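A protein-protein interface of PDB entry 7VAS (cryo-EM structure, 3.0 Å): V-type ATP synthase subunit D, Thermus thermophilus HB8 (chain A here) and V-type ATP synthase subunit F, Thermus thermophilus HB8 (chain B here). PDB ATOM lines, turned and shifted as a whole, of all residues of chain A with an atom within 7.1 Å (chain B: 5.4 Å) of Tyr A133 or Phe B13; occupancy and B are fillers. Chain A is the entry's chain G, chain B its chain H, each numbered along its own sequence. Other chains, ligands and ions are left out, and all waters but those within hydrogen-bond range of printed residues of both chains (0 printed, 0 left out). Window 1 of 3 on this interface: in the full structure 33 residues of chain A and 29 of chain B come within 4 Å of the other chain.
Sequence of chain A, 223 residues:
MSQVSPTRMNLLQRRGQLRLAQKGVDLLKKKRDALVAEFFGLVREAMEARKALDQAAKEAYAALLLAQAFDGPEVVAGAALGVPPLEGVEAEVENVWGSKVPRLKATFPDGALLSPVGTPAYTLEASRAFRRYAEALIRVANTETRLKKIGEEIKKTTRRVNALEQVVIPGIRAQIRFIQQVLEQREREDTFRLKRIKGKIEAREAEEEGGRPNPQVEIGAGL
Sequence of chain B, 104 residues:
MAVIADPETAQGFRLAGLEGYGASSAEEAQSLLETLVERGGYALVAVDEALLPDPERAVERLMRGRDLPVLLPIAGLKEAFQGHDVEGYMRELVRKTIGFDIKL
OH of Tyr A61 sits at hydrogen-bond distance from OG1 of Thr B9 (2.9 Å).
The side-chain hydroxyl (OG) of Ser A127 is in hydrogen-bond range of the backbone carbonyl oxygen (O) of Leu B15 (3.4 Å).
The guanidinium group (NE) of Arg A131 sits at hydrogen-bond distance from the backbone carbonyl oxygen (O) of Ala B16 (2.7 Å).
The backbone carbonyl oxygen (O) of Phe B13 is in hydrogen-bond range of the backbone NH (N) of Leu B18, at 2.9 Å.
Among the printed residues, pairs that only touch across the chains: Leu A53 with Ile B74 (3.8 Å), Ala A80 with Leu B15 (3.4 Å), Phe A130 with Gly B12 (3.3 Å), Phe A130 with Phe B13 (3.5 Å), Phe A130 with Ala B16 (3.5 Å), Tyr A133 with Phe B13 (3.5 Å) and Tyr A133 with Ile B74 (3.1 Å).
Tyr A133 touches two residues of chain B.
Of the printed residues of chain A, Phe B13 touches Phe A130 (3.5 Å) and Tyr A133 (3.5 Å).
Printed residues of chain B within 4 Å of Ser A127: Leu B15 (3.4 Å).
Of the printed residues of chain A, Ala B16 touches Phe A130 and Arg A131.
Printed residues of chain B within 4 Å of Tyr A61: Thr B9.
Of the printed residues of chain B, Ala A80 touches Leu B15 (3.4 Å).
Of the printed residues of chain A, Thr B9 touches Tyr A61.
Arg A132 touches none of the printed residues of chain B.
Of the 23 printed residues of chain A, 7 touch a printed residue of chain B.
Along chain B the printed residues that touch a printed residue of chain A span positions 9 to 74.
Among the printed residues, 10 pairs touch across the chains.
Among the printed residues, no Asp or Glu carboxylate lies within 4 Å of a Lys or Arg side-chain nitrogen of the other chain.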
ATOM      1  N   LEU A  53      17.696  -9.021 -14.453  1.00  0.00           N
ATOM      2  CA  LEU A  53      19.088  -9.433 -14.313  1.00  0.00           C
ATOM      3  C   LEU A  53      19.753  -9.592 -15.671  1.00  0.00           C
ATOM      4  O   LEU A  53      20.925  -9.243 -15.837  1.00  0.00           O
ATOM      5  CB  LEU A  53      19.183 -10.736 -13.523  1.00  0.00           C
ATOM      6  CG  LEU A  53      20.617 -11.229 -13.308  1.00  0.00           C
ATOM      7  CD1 LEU A  53      21.378 -10.271 -12.408  1.00  0.00           C
ATOM      8  CD2 LEU A  53      20.641 -12.637 -12.742  1.00  0.00           C
ATOM      9  N   ASP A  54      19.027 -10.133 -16.651  1.00  0.00           N
ATOM     10  CA  ASP A  54      19.591 -10.283 -17.989  1.00  0.00           C
ATOM     11  C   ASP A  54      19.923  -8.930 -18.606  1.00  0.00           C
ATOM     12  O   ASP A  54      20.986  -8.760 -19.219  1.00  0.00           O
ATOM     13  CB  ASP A  54      18.620 -11.055 -18.880  1.00  0.00           C
ATOM     14  CG  ASP A  54      19.167 -11.288 -20.271  1.00  0.00           C
ATOM     15  OD1 ASP A  54      20.397 -11.460 -20.408  1.00  0.00           O
ATOM     16  OD2 ASP A  54      18.366 -11.300 -21.229  1.00  0.00           O
ATOM     17  N   ALA A  56      20.592  -6.108 -16.988  1.00  0.00           N
ATOM     18  CA  ALA A  56      21.743  -5.567 -16.272  1.00  0.00           C
ATOM     19  C   ALA A  56      23.029  -6.262 -16.700  1.00  0.00           C
ATOM     20  O   ALA A  56      24.079  -5.621 -16.822  1.00  0.00           O
ATOM     21  CB  ALA A  56      21.536  -5.692 -14.764  1.00  0.00           C
ATOM     22  N   ALA A  57      22.964  -7.574 -16.936  1.00  0.00           N
ATOM     23  CA  ALA A  57      24.129  -8.308 -17.412  1.00  0.00           C
ATOM     24  C   ALA A  57      24.582  -7.798 -18.769  1.00  0.00           C
ATOM     25  O   ALA A  57      25.783  -7.615 -19.005  1.00  0.00           O
ATOM     26  CB  ALA A  57      23.810  -9.800 -17.488  1.00  0.00           C
ATOM     27  N   LYS A  58      23.632  -7.571 -19.679  1.00  0.00           N
ATOM     28  CA  LYS A  58      23.985  -7.056 -20.998  1.00  0.00           C
ATOM     29  C   LYS A  58      24.695  -5.714 -20.886  1.00  0.00           C
ATOM     30  O   LYS A  58      25.764  -5.512 -21.477  1.00  0.00           O
ATOM     31  CB  LYS A  58      22.733  -6.928 -21.867  1.00  0.00           C
ATOM     32  CG  LYS A  58      22.176  -8.249 -22.359  1.00  0.00           C
ATOM     33  CD  LYS A  58      20.808  -8.059 -22.994  1.00  0.00           C
ATOM     34  CE  LYS A  58      20.905  -7.249 -24.276  1.00  0.00           C
ATOM     35  NZ  LYS A  58      21.488  -8.046 -25.390  1.00  0.00           N
ATOM     36  N   GLU A  59      24.121  -4.782 -20.116  1.00  0.00           N
ATOM     37  CA  GLU A  59      24.736  -3.459 -20.038  1.00  0.00           C
ATOM     38  C   GLU A  59      26.094  -3.519 -19.341  1.00  0.00           C
ATOM     39  O   GLU A  59      27.039  -2.834 -19.754  1.00  0.00           O
ATOM     40  CB  GLU A  59      23.802  -2.461 -19.346  1.00  0.00           C
ATOM     41  CG  GLU A  59      23.450  -2.756 -17.900  1.00  0.00           C
ATOM     42  CD  GLU A  59      24.467  -2.191 -16.924  1.00  0.00           C
ATOM     43  OE1 GLU A  59      25.223  -1.278 -17.315  1.00  0.00           O
ATOM     44  OE2 GLU A  59      24.508  -2.657 -15.766  1.00  0.00           O
ATOM     45  N   ALA A  60      26.221  -4.348 -18.301  1.00  0.00           N
ATOM     46  CA  ALA A  60      27.488  -4.447 -17.585  1.00  0.00           C
ATOM     47  C   ALA A  60      28.580  -5.047 -18.460  1.00  0.00           C
ATOM     48  O   ALA A  60      29.725  -4.584 -18.435  1.00  0.00           O
ATOM     49  CB  ALA A  60      27.309  -5.271 -16.311  1.00  0.00           C
ATOM     50  N   TYR A  61      28.251  -6.080 -19.239  1.00  0.00           N
ATOM     51  CA  TYR A  61      29.254  -6.672 -20.115  1.00  0.00           C
ATOM     52  C   TYR A  61      29.632  -5.720 -21.242  1.00  0.00           C
ATOM     53  O   TYR A  61      30.805  -5.649 -21.636  1.00  0.00           O
ATOM     54  CB  TYR A  61      28.747  -8.003 -20.666  1.00  0.00           C
ATOM     55  CG  TYR A  61      28.996  -9.157 -19.725  1.00  0.00           C
ATOM     56  CD1 TYR A  61      30.244  -9.345 -19.147  1.00  0.00           C
ATOM     57  CD2 TYR A  61      27.983 -10.048 -19.403  1.00  0.00           C
ATOM     58  CE1 TYR A  61      30.479 -10.392 -18.281  1.00  0.00           C
ATOM     59  CE2 TYR A  61      28.209 -11.101 -18.536  1.00  0.00           C
ATOM     60  CZ  TYR A  61      29.459 -11.269 -17.980  1.00  0.00           C
ATOM     61  OH  TYR A  61      29.692 -12.315 -17.117  1.00  0.00           O
ATOM     62  N   LEU A  64      32.040  -3.372 -19.687  1.00  0.00           N
ATOM     63  CA  LEU A  64      33.331  -3.987 -19.393  1.00  0.00           C
ATOM     64  C   LEU A  64      34.175  -4.139 -20.652  1.00  0.00           C
ATOM     65  O   LEU A  64      35.370  -3.824 -20.652  1.00  0.00           O
ATOM     66  CB  LEU A  64      33.135  -5.346 -18.723  1.00  0.00           C
ATOM     67  CG  LEU A  64      34.447  -6.047 -18.358  1.00  0.00           C
ATOM     68  CD1 LEU A  64      35.194  -5.264 -17.288  1.00  0.00           C
ATOM     69  CD2 LEU A  64      34.210  -7.484 -17.919  1.00  0.00           C
ATOM     70  N   ALA A  80      41.559  -3.405  -9.991  1.00  0.00           N
ATOM     71  CA  ALA A  80      40.983  -4.486  -9.200  1.00  0.00           C
ATOM     72  C   ALA A  80      41.897  -4.889  -8.052  1.00  0.00           C
ATOM     73  O   ALA A  80      41.416  -5.320  -6.998  1.00  0.00           O
ATOM     74  CB  ALA A  80      40.685  -5.691 -10.091  1.00  0.00           C
ATOM     75  N   SER A 127      32.805  -0.634 -13.063  1.00  0.00           N
ATOM     76  CA  SER A 127      32.621  -1.148 -11.708  1.00  0.00           C
ATOM     77  C   SER A 127      31.197  -0.926 -11.213  1.00  0.00           C
ATOM     78  O   SER A 127      30.610  -1.811 -10.580  1.00  0.00           O
ATOM     79  CB  SER A 127      33.629  -0.501 -10.760  1.00  0.00           C
ATOM     80  OG  SER A 127      33.663  -1.182  -9.517  1.00  0.00           O
ATOM     81  N   ARG A 128      30.626   0.249 -11.487  1.00  0.00           N
ATOM     82  CA  ARG A 128      29.246   0.514 -11.088  1.00  0.00           C
ATOM     83  C   ARG A 128      28.281  -0.426 -11.800  1.00  0.00           C
ATOM     84  O   ARG A 128      27.270  -0.853 -11.223  1.00  0.00           O
ATOM     85  CB  ARG A 128      28.899   1.972 -11.378  1.00  0.00           C
ATOM     86  CG  ARG A 128      29.737   2.959 -10.585  1.00  0.00           C
ATOM     87  CD  ARG A 128      29.727   4.335 -11.222  1.00  0.00           C
ATOM     88  NE  ARG A 128      28.388   4.908 -11.275  1.00  0.00           N
ATOM     89  CZ  ARG A 128      28.079   6.024 -11.920  1.00  0.00           C
ATOM     90  NH1 ARG A 128      28.995   6.719 -12.575  1.00  0.00           N
ATOM     91  NH2 ARG A 128      26.822   6.455 -11.904  1.00  0.00           N
ATOM     92  N   ALA A 129      28.578  -0.758 -13.058  1.00  0.00           N
ATOM     93  CA  ALA A 129      27.767  -1.731 -13.777  1.00  0.00           C
ATOM     94  C   ALA A 129      27.797  -3.084 -13.082  1.00  0.00           C
ATOM     95  O   ALA A 129      26.764  -3.748 -12.959  1.00  0.00           O
ATOM     96  CB  ALA A 129      28.251  -1.852 -15.220  1.00  0.00           C
ATOM     97  N   PHE A 130      28.970  -3.501 -12.605  1.00  0.00           N
ATOM     98  CA  PHE A 130      29.056  -4.767 -11.885  1.00  0.00           C
ATOM     99  C   PHE A 130      28.364  -4.692 -10.527  1.00  0.00           C
ATOM    100  O   PHE A 130      27.822  -5.697 -10.054  1.00  0.00           O
ATOM    101  CB  PHE A 130      30.518  -5.177 -11.731  1.00  0.00           C
ATOM    102  CG  PHE A 130      31.041  -5.984 -12.882  1.00  0.00           C
ATOM    103  CD1 PHE A 130      31.288  -5.389 -14.107  1.00  0.00           C
ATOM    104  CD2 PHE A 130      31.278  -7.342 -12.744  1.00  0.00           C
ATOM    105  CE1 PHE A 130      31.767  -6.129 -15.169  1.00  0.00           C
ATOM    106  CE2 PHE A 130      31.756  -8.089 -13.804  1.00  0.00           C
ATOM    107  CZ  PHE A 130      32.001  -7.482 -15.018  1.00  0.00           C
ATOM    108  N   ARG A 131      28.366  -3.520  -9.888  1.00  0.00           N
ATOM    109  CA  ARG A 131      27.621  -3.371  -8.641  1.00  0.00           C
ATOM    110  C   ARG A 131      26.123  -3.533  -8.871  1.00  0.00           C
ATOM    111  O   ARG A 131      25.437  -4.216  -8.098  1.00  0.00           O
ATOM    112  CB  ARG A 131      27.924  -2.014  -8.005  1.00  0.00           C
ATOM    113  CG  ARG A 131      28.985  -2.065  -6.920  1.00  0.00           C
ATOM    114  CD  ARG A 131      30.331  -2.472  -7.493  1.00  0.00           C
ATOM    115  NE  ARG A 131      31.289  -2.856  -6.463  1.00  0.00           N
ATOM    116  CZ  ARG A 131      32.139  -2.020  -5.884  1.00  0.00           C
ATOM    117  NH1 ARG A 131      32.167  -0.735  -6.197  1.00  0.00           N
ATOM    118  NH2 ARG A 131      32.984  -2.485  -4.969  1.00  0.00           N
ATOM    119  N   ARG A 132      25.601  -2.911  -9.931  1.00  0.00           N
ATOM    120  CA  ARG A 132      24.194  -3.101 -10.276  1.00  0.00           C
ATOM    121  C   ARG A 132      23.915  -4.554 -10.648  1.00  0.00           C
ATOM    122  O   ARG A 132      22.870  -5.115 -10.286  1.00  0.00           O
ATOM    123  CB  ARG A 132      23.802  -2.152 -11.408  1.00  0.00           C
ATOM    124  CG  ARG A 132      23.936  -0.688 -11.019  1.00  0.00           C
ATOM    125  CD  ARG A 132      23.402   0.244 -12.092  1.00  0.00           C
ATOM    126  NE  ARG A 132      24.081   0.073 -13.371  1.00  0.00           N
ATOM    127  CZ  ARG A 132      25.201   0.695 -13.711  1.00  0.00           C
ATOM    128  NH1 ARG A 132      25.823   1.509 -12.872  1.00  0.00           N
ATOM    129  NH2 ARG A 132      25.710   0.499 -14.924  1.00  0.00           N
ATOM    130  N   TYR A 133      24.853  -5.177 -11.362  1.00  0.00           N
ATOM    131  CA  TYR A 133      24.788  -6.602 -11.658  1.00  0.00           C
ATOM    132  C   TYR A 133      24.583  -7.418 -10.388  1.00  0.00           C
ATOM    133  O   TYR A 133      23.675  -8.254 -10.308  1.00  0.00           O
ATOM    134  CB  TYR A 133      26.086  -7.005 -12.359  1.00  0.00           C
ATOM    135  CG  TYR A 133      26.133  -8.388 -12.950  1.00  0.00           C
ATOM    136  CD1 TYR A 133      25.850  -8.596 -14.288  1.00  0.00           C
ATOM    137  CD2 TYR A 133      26.493  -9.483 -12.179  1.00  0.00           C
ATOM    138  CE1 TYR A 133      25.911  -9.851 -14.840  1.00  0.00           C
ATOM    139  CE2 TYR A 133      26.550 -10.747 -12.724  1.00  0.00           C
ATOM    140  CZ  TYR A 133      26.255 -10.925 -14.057  1.00  0.00           C
ATOM    141  OH  TYR A 133      26.309 -12.176 -14.620  1.00  0.00           O
ATOM    142  N   ALA A 134      25.415  -7.171  -9.375  1.00  0.00           N
ATOM    143  CA  ALA A 134      25.338  -7.944  -8.137  1.00  0.00           C
ATOM    144  C   ALA A 134      24.047  -7.663  -7.375  1.00  0.00           C
ATOM    145  O   ALA A 134      23.444  -8.584  -6.803  1.00  0.00           O
ATOM    146  CB  ALA A 134      26.552  -7.647  -7.259  1.00  0.00           C
ATOM    147  N   GLU A 135      23.611  -6.401  -7.334  1.00  0.00           N
ATOM    148  CA  GLU A 135      22.398  -6.095  -6.584  1.00  0.00           C
ATOM    149  C   GLU A 135      21.143  -6.595  -7.290  1.00  0.00           C
ATOM    150  O   GLU A 135      20.085  -6.678  -6.656  1.00  0.00           O
ATOM    151  CB  GLU A 135      22.291  -4.594  -6.300  1.00  0.00           C
ATOM    152  CG  GLU A 135      22.226  -3.703  -7.520  1.00  0.00           C
ATOM    153  CD  GLU A 135      20.818  -3.522  -8.047  1.00  0.00           C
ATOM    154  OE1 GLU A 135      19.860  -3.836  -7.310  1.00  0.00           O
ATOM    155  OE2 GLU A 135      20.671  -3.066  -9.200  1.00  0.00           O
ATOM    156  N   ALA A 136      21.225  -6.913  -8.584  1.00  0.00           N
ATOM    157  CA  ALA A 136      20.120  -7.629  -9.217  1.00  0.00           C
ATOM    158  C   ALA A 136      20.246  -9.136  -9.009  1.00  0.00           C
ATOM    159  O   ALA A 136      19.235  -9.840  -8.850  1.00  0.00           O
ATOM    160  CB  ALA A 136      20.061  -7.294 -10.707  1.00  0.00           C
ATOM    161  N   LEU A 137      21.482  -9.640  -9.001  1.00  0.00           N
ATOM    162  CA  LEU A 137      21.708 -11.068  -8.810  1.00  0.00           C
ATOM    163  C   LEU A 137      21.222 -11.527  -7.442  1.00  0.00           C
ATOM    164  O   LEU A 137      20.678 -12.630  -7.306  1.00  0.00           O
ATOM    165  CB  LEU A 137      23.192 -11.382  -8.993  1.00  0.00           C
ATOM    166  CG  LEU A 137      23.618 -12.846  -8.901  1.00  0.00           C
ATOM    167  CD1 LEU A 137      23.388 -13.547 -10.228  1.00  0.00           C
ATOM    168  CD2 LEU A 137      25.076 -12.947  -8.485  1.00  0.00           C
ATOM    169  N   ILE A 138      21.416 -10.698  -6.413  1.00  0.00           N
ATOM    170  CA  ILE A 138      20.960 -11.076  -5.076  1.00  0.00           C
ATOM    171  C   ILE A 138      19.439 -11.196  -5.041  1.00  0.00           C
ATOM    172  O   ILE A 138      18.888 -12.119  -4.427  1.00  0.00           O
ATOM    173  CB  ILE A 138      21.479 -10.082  -4.020  1.00  0.00           C
ATOM    174  CG1 ILE A 138      21.061  -8.653  -4.363  1.00  0.00           C
ATOM    175  CG2 ILE A 138      22.989 -10.188  -3.891  1.00  0.00           C
ATOM    176  CD1 ILE A 138      20.853  -7.773  -3.156  1.00  0.00           C
ATOM    177  N   ARG A 139      18.738 -10.267  -5.697  1.00  0.00           N
ATOM    178  CA  ARG A 139      17.282 -10.346  -5.764  1.00  0.00           C
ATOM    179  C   ARG A 139      16.836 -11.612  -6.479  1.00  0.00           C
ATOM    180  O   ARG A 139      15.896 -12.292  -6.038  1.00  0.00           O
ATOM    181  CB  ARG A 139      16.726  -9.111  -6.469  1.00  0.00           C
ATOM    182  CG  ARG A 139      15.229  -8.930  -6.323  1.00  0.00           C
ATOM    183  CD  ARG A 139      14.825  -7.495  -6.609  1.00  0.00           C
ATOM    184  NE  ARG A 139      14.906  -7.172  -8.029  1.00  0.00           N
ATOM    185  CZ  ARG A 139      13.872  -7.186  -8.860  1.00  0.00           C
ATOM    186  NH1 ARG A 139      12.657  -7.508  -8.447  1.00  0.00           N
ATOM    187  NH2 ARG A 139      14.062  -6.864 -10.137  1.00  0.00           N
ATOM    188  N   VAL B   3      32.030 -15.990  -7.168  1.00  0.00           N
ATOM    189  CA  VAL B   3      31.484 -16.204  -8.504  1.00  0.00           C
ATOM    190  C   VAL B   3      32.401 -17.148  -9.268  1.00  0.00           C
ATOM    191  O   VAL B   3      33.628 -17.010  -9.220  1.00  0.00           O
ATOM    192  CB  VAL B   3      31.313 -14.879  -9.277  1.00  0.00           C
ATOM    193  CG1 VAL B   3      30.721 -15.142 -10.652  1.00  0.00           C
ATOM    194  CG2 VAL B   3      30.439 -13.912  -8.499  1.00  0.00           C
ATOM    195  N   ALA B   5      32.954 -18.405 -13.151  1.00  0.00           N
ATOM    196  CA  ALA B   5      32.638 -18.147 -14.550  1.00  0.00           C
ATOM    197  C   ALA B   5      33.945 -18.149 -15.334  1.00  0.00           C
ATOM    198  O   ALA B   5      34.988 -18.581 -14.830  1.00  0.00           O
ATOM    199  CB  ALA B   5      31.868 -16.832 -14.707  1.00  0.00           C
ATOM    200  N   THR B   9      35.528 -12.528 -17.218  1.00  0.00           N
ATOM    201  CA  THR B   9      34.567 -11.825 -16.377  1.00  0.00           C
ATOM    202  C   THR B   9      34.907 -11.935 -14.897  1.00  0.00           C
ATOM    203  O   THR B   9      34.430 -11.115 -14.102  1.00  0.00           O
ATOM    204  CB  THR B   9      33.152 -12.347 -16.631  1.00  0.00           C
ATOM    205  OG1 THR B   9      32.206 -11.508 -15.959  1.00  0.00           O
ATOM    206  CG2 THR B   9      33.008 -13.768 -16.124  1.00  0.00           C
ATOM    207  N   ALA B  10      35.712 -12.927 -14.508  1.00  0.00           N
ATOM    208  CA  ALA B  10      36.188 -12.984 -13.132  1.00  0.00           C
ATOM    209  C   ALA B  10      37.008 -11.750 -12.790  1.00  0.00           C
ATOM    210  O   ALA B  10      36.994 -11.292 -11.642  1.00  0.00           O
ATOM    211  CB  ALA B  10      37.006 -14.255 -12.906  1.00  0.00           C
ATOM    212  N   GLN B  11      37.712 -11.191 -13.776  1.00  0.00           N
ATOM    213  CA  GLN B  11      38.418  -9.934 -13.563  1.00  0.00           C
ATOM    214  C   GLN B  11      37.446  -8.812 -13.230  1.00  0.00           C
ATOM    215  O   GLN B  11      37.697  -8.014 -12.320  1.00  0.00           O
ATOM    216  CB  GLN B  11      39.244  -9.585 -14.799  1.00  0.00           C
ATOM    217  CG  GLN B  11      40.142  -8.374 -14.631  1.00  0.00           C
ATOM    218  CD  GLN B  11      40.921  -8.054 -15.892  1.00  0.00           C
ATOM    219  OE1 GLN B  11      40.375  -8.079 -16.995  1.00  0.00           O
ATOM    220  NE2 GLN B  11      42.204  -7.750 -15.735  1.00  0.00           N
ATOM    221  N   GLY B  12      36.322  -8.741 -13.944  1.00  0.00           N
ATOM    222  CA  GLY B  12      35.322  -7.734 -13.625  1.00  0.00           C
ATOM    223  C   GLY B  12      34.701  -7.939 -12.257  1.00  0.00           C
ATOM    224  O   GLY B  12      34.458  -6.976 -11.523  1.00  0.00           O
ATOM    225  N   PHE B  13      34.426  -9.195 -11.896  1.00  0.00           N
ATOM    226  CA  PHE B  13      33.868  -9.474 -10.576  1.00  0.00           C
ATOM    227  C   PHE B  13      34.840  -9.076  -9.473  1.00  0.00           C
ATOM    228  O   PHE B  13      34.431  -8.523  -8.445  1.00  0.00           O
ATOM    229  CB  PHE B  13      33.490 -10.950 -10.466  1.00  0.00           C
ATOM    230  CG  PHE B  13      32.195 -11.289 -11.144  1.00  0.00           C
ATOM    231  CD1 PHE B  13      31.002 -10.750 -10.695  1.00  0.00           C
ATOM    232  CD2 PHE B  13      32.170 -12.135 -12.240  1.00  0.00           C
ATOM    233  CE1 PHE B  13      29.809 -11.053 -11.319  1.00  0.00           C
ATOM    234  CE2 PHE B  13      30.980 -12.441 -12.870  1.00  0.00           C
ATOM    235  CZ  PHE B  13      29.798 -11.901 -12.408  1.00  0.00           C
ATOM    236  N   ARG B  14      36.132  -9.350  -9.667  1.00  0.00           N
ATOM    237  CA  ARG B  14      37.140  -8.873  -8.726  1.00  0.00           C
ATOM    238  C   ARG B  14      37.182  -7.351  -8.698  1.00  0.00           C
ATOM    239  O   ARG B  14      37.383  -6.744  -7.639  1.00  0.00           O
ATOM    240  CB  ARG B  14      38.508  -9.448  -9.090  1.00  0.00           C
ATOM    241  CG  ARG B  14      38.704 -10.893  -8.658  1.00  0.00           C
ATOM    242  CD  ARG B  14      40.007 -11.471  -9.192  1.00  0.00           C
ATOM    243  NE  ARG B  14      39.797 -12.300 -10.373  1.00  0.00           N
ATOM    244  CZ  ARG B  14      40.313 -12.048 -11.569  1.00  0.00           C
ATOM    245  NH1 ARG B  14      41.085 -10.994 -11.780  1.00  0.00           N
ATOM    246  NH2 ARG B  14      40.050 -12.874 -12.577  1.00  0.00           N
ATOM    247  N   LEU B  15      36.995  -6.718  -9.859  1.00  0.00           N
ATOM    248  CA  LEU B  15      36.932  -5.263  -9.927  1.00  0.00           C
ATOM    249  C   LEU B  15      35.760  -4.717  -9.127  1.00  0.00           C
ATOM    250  O   LEU B  15      35.826  -3.595  -8.612  1.00  0.00           O
ATOM    251  CB  LEU B  15      36.832  -4.820 -11.386  1.00  0.00           C
ATOM    252  CG  LEU B  15      37.084  -3.350 -11.716  1.00  0.00           C
ATOM    253  CD1 LEU B  15      38.560  -3.019 -11.587  1.00  0.00           C
ATOM    254  CD2 LEU B  15      36.580  -3.031 -13.112  1.00  0.00           C
ATOM    255  N   ALA B  16      34.683  -5.489  -9.014  1.00  0.00           N
ATOM    256  CA  ALA B  16      33.526  -5.085  -8.227  1.00  0.00           C
ATOM    257  C   ALA B  16      33.688  -5.371  -6.740  1.00  0.00           C
ATOM    258  O   ALA B  16      32.795  -5.025  -5.959  1.00  0.00           O
ATOM    259  CB  ALA B  16      32.268  -5.784  -8.742  1.00  0.00           C
ATOM    260  N   GLY B  17      34.796  -5.985  -6.330  1.00  0.00           N
ATOM    261  CA  GLY B  17      34.981  -6.403  -4.960  1.00  0.00           C
ATOM    262  C   GLY B  17      34.521  -7.813  -4.663  1.00  0.00           C
ATOM    263  O   GLY B  17      34.757  -8.303  -3.552  1.00  0.00           O
ATOM    264  N   LEU B  18      33.872  -8.476  -5.614  1.00  0.00           N
ATOM    265  CA  LEU B  18      33.472  -9.862  -5.444  1.00  0.00           C
ATOM    266  C   LEU B  18      34.671 -10.787  -5.633  1.00  0.00           C
ATOM    267  O   LEU B  18      35.667 -10.436  -6.270  1.00  0.00           O
ATOM    268  CB  LEU B  18      32.362 -10.227  -6.430  1.00  0.00           C
ATOM    269  CG  LEU B  18      30.924  -9.889  -6.024  1.00  0.00           C
ATOM    270  CD1 LEU B  18      30.661  -8.395  -6.121  1.00  0.00           C
ATOM    271  CD2 LEU B  18      29.933 -10.660  -6.881  1.00  0.00           C
ATOM    272  N   GLU B  19      34.564 -11.987  -5.062  1.00  0.00           N
ATOM    273  CA  GLU B  19      35.637 -12.979  -5.137  1.00  0.00           C
ATOM    274  C   GLU B  19      35.510 -13.767  -6.441  1.00  0.00           C
ATOM    275  O   GLU B  19      35.140 -14.942  -6.475  1.00  0.00           O
ATOM    276  CB  GLU B  19      35.603 -13.894  -3.922  1.00  0.00           C
ATOM    277  CG  GLU B  19      35.597 -13.155  -2.596  1.00  0.00           C
ATOM    278  CD  GLU B  19      35.975 -14.045  -1.431  1.00  0.00           C
ATOM    279  OE1 GLU B  19      35.632 -15.245  -1.462  1.00  0.00           O
ATOM    280  OE2 GLU B  19      36.616 -13.544  -0.483  1.00  0.00           O
ATOM    281  N   GLY B  20      35.823 -13.083  -7.538  1.00  0.00           N
ATOM    282  CA  GLY B  20      35.748 -13.712  -8.846  1.00  0.00           C
ATOM    283  C   GLY B  20      36.801 -14.796  -8.995  1.00  0.00           C
ATOM    284  O   GLY B  20      37.981 -14.587  -8.686  1.00  0.00           O
ATOM    285  N   ILE B  74      24.428 -18.722 -13.932  1.00  0.00           N
ATOM    286  CA  ILE B  74      24.411 -17.458 -14.658  1.00  0.00           C
ATOM    287  C   ILE B  74      24.866 -17.707 -16.090  1.00  0.00           C
ATOM    288  O   ILE B  74      25.658 -18.615 -16.362  1.00  0.00           O
ATOM    289  CB  ILE B  74      25.283 -16.385 -13.965  1.00  0.00           C
ATOM    290  CG1 ILE B  74      24.949 -14.997 -14.513  1.00  0.00           C
ATOM    291  CG2 ILE B  74      26.762 -16.697 -14.127  1.00  0.00           C
ATOM    292  CD1 ILE B  74      23.519 -14.574 -14.260  1.00  0.00           C
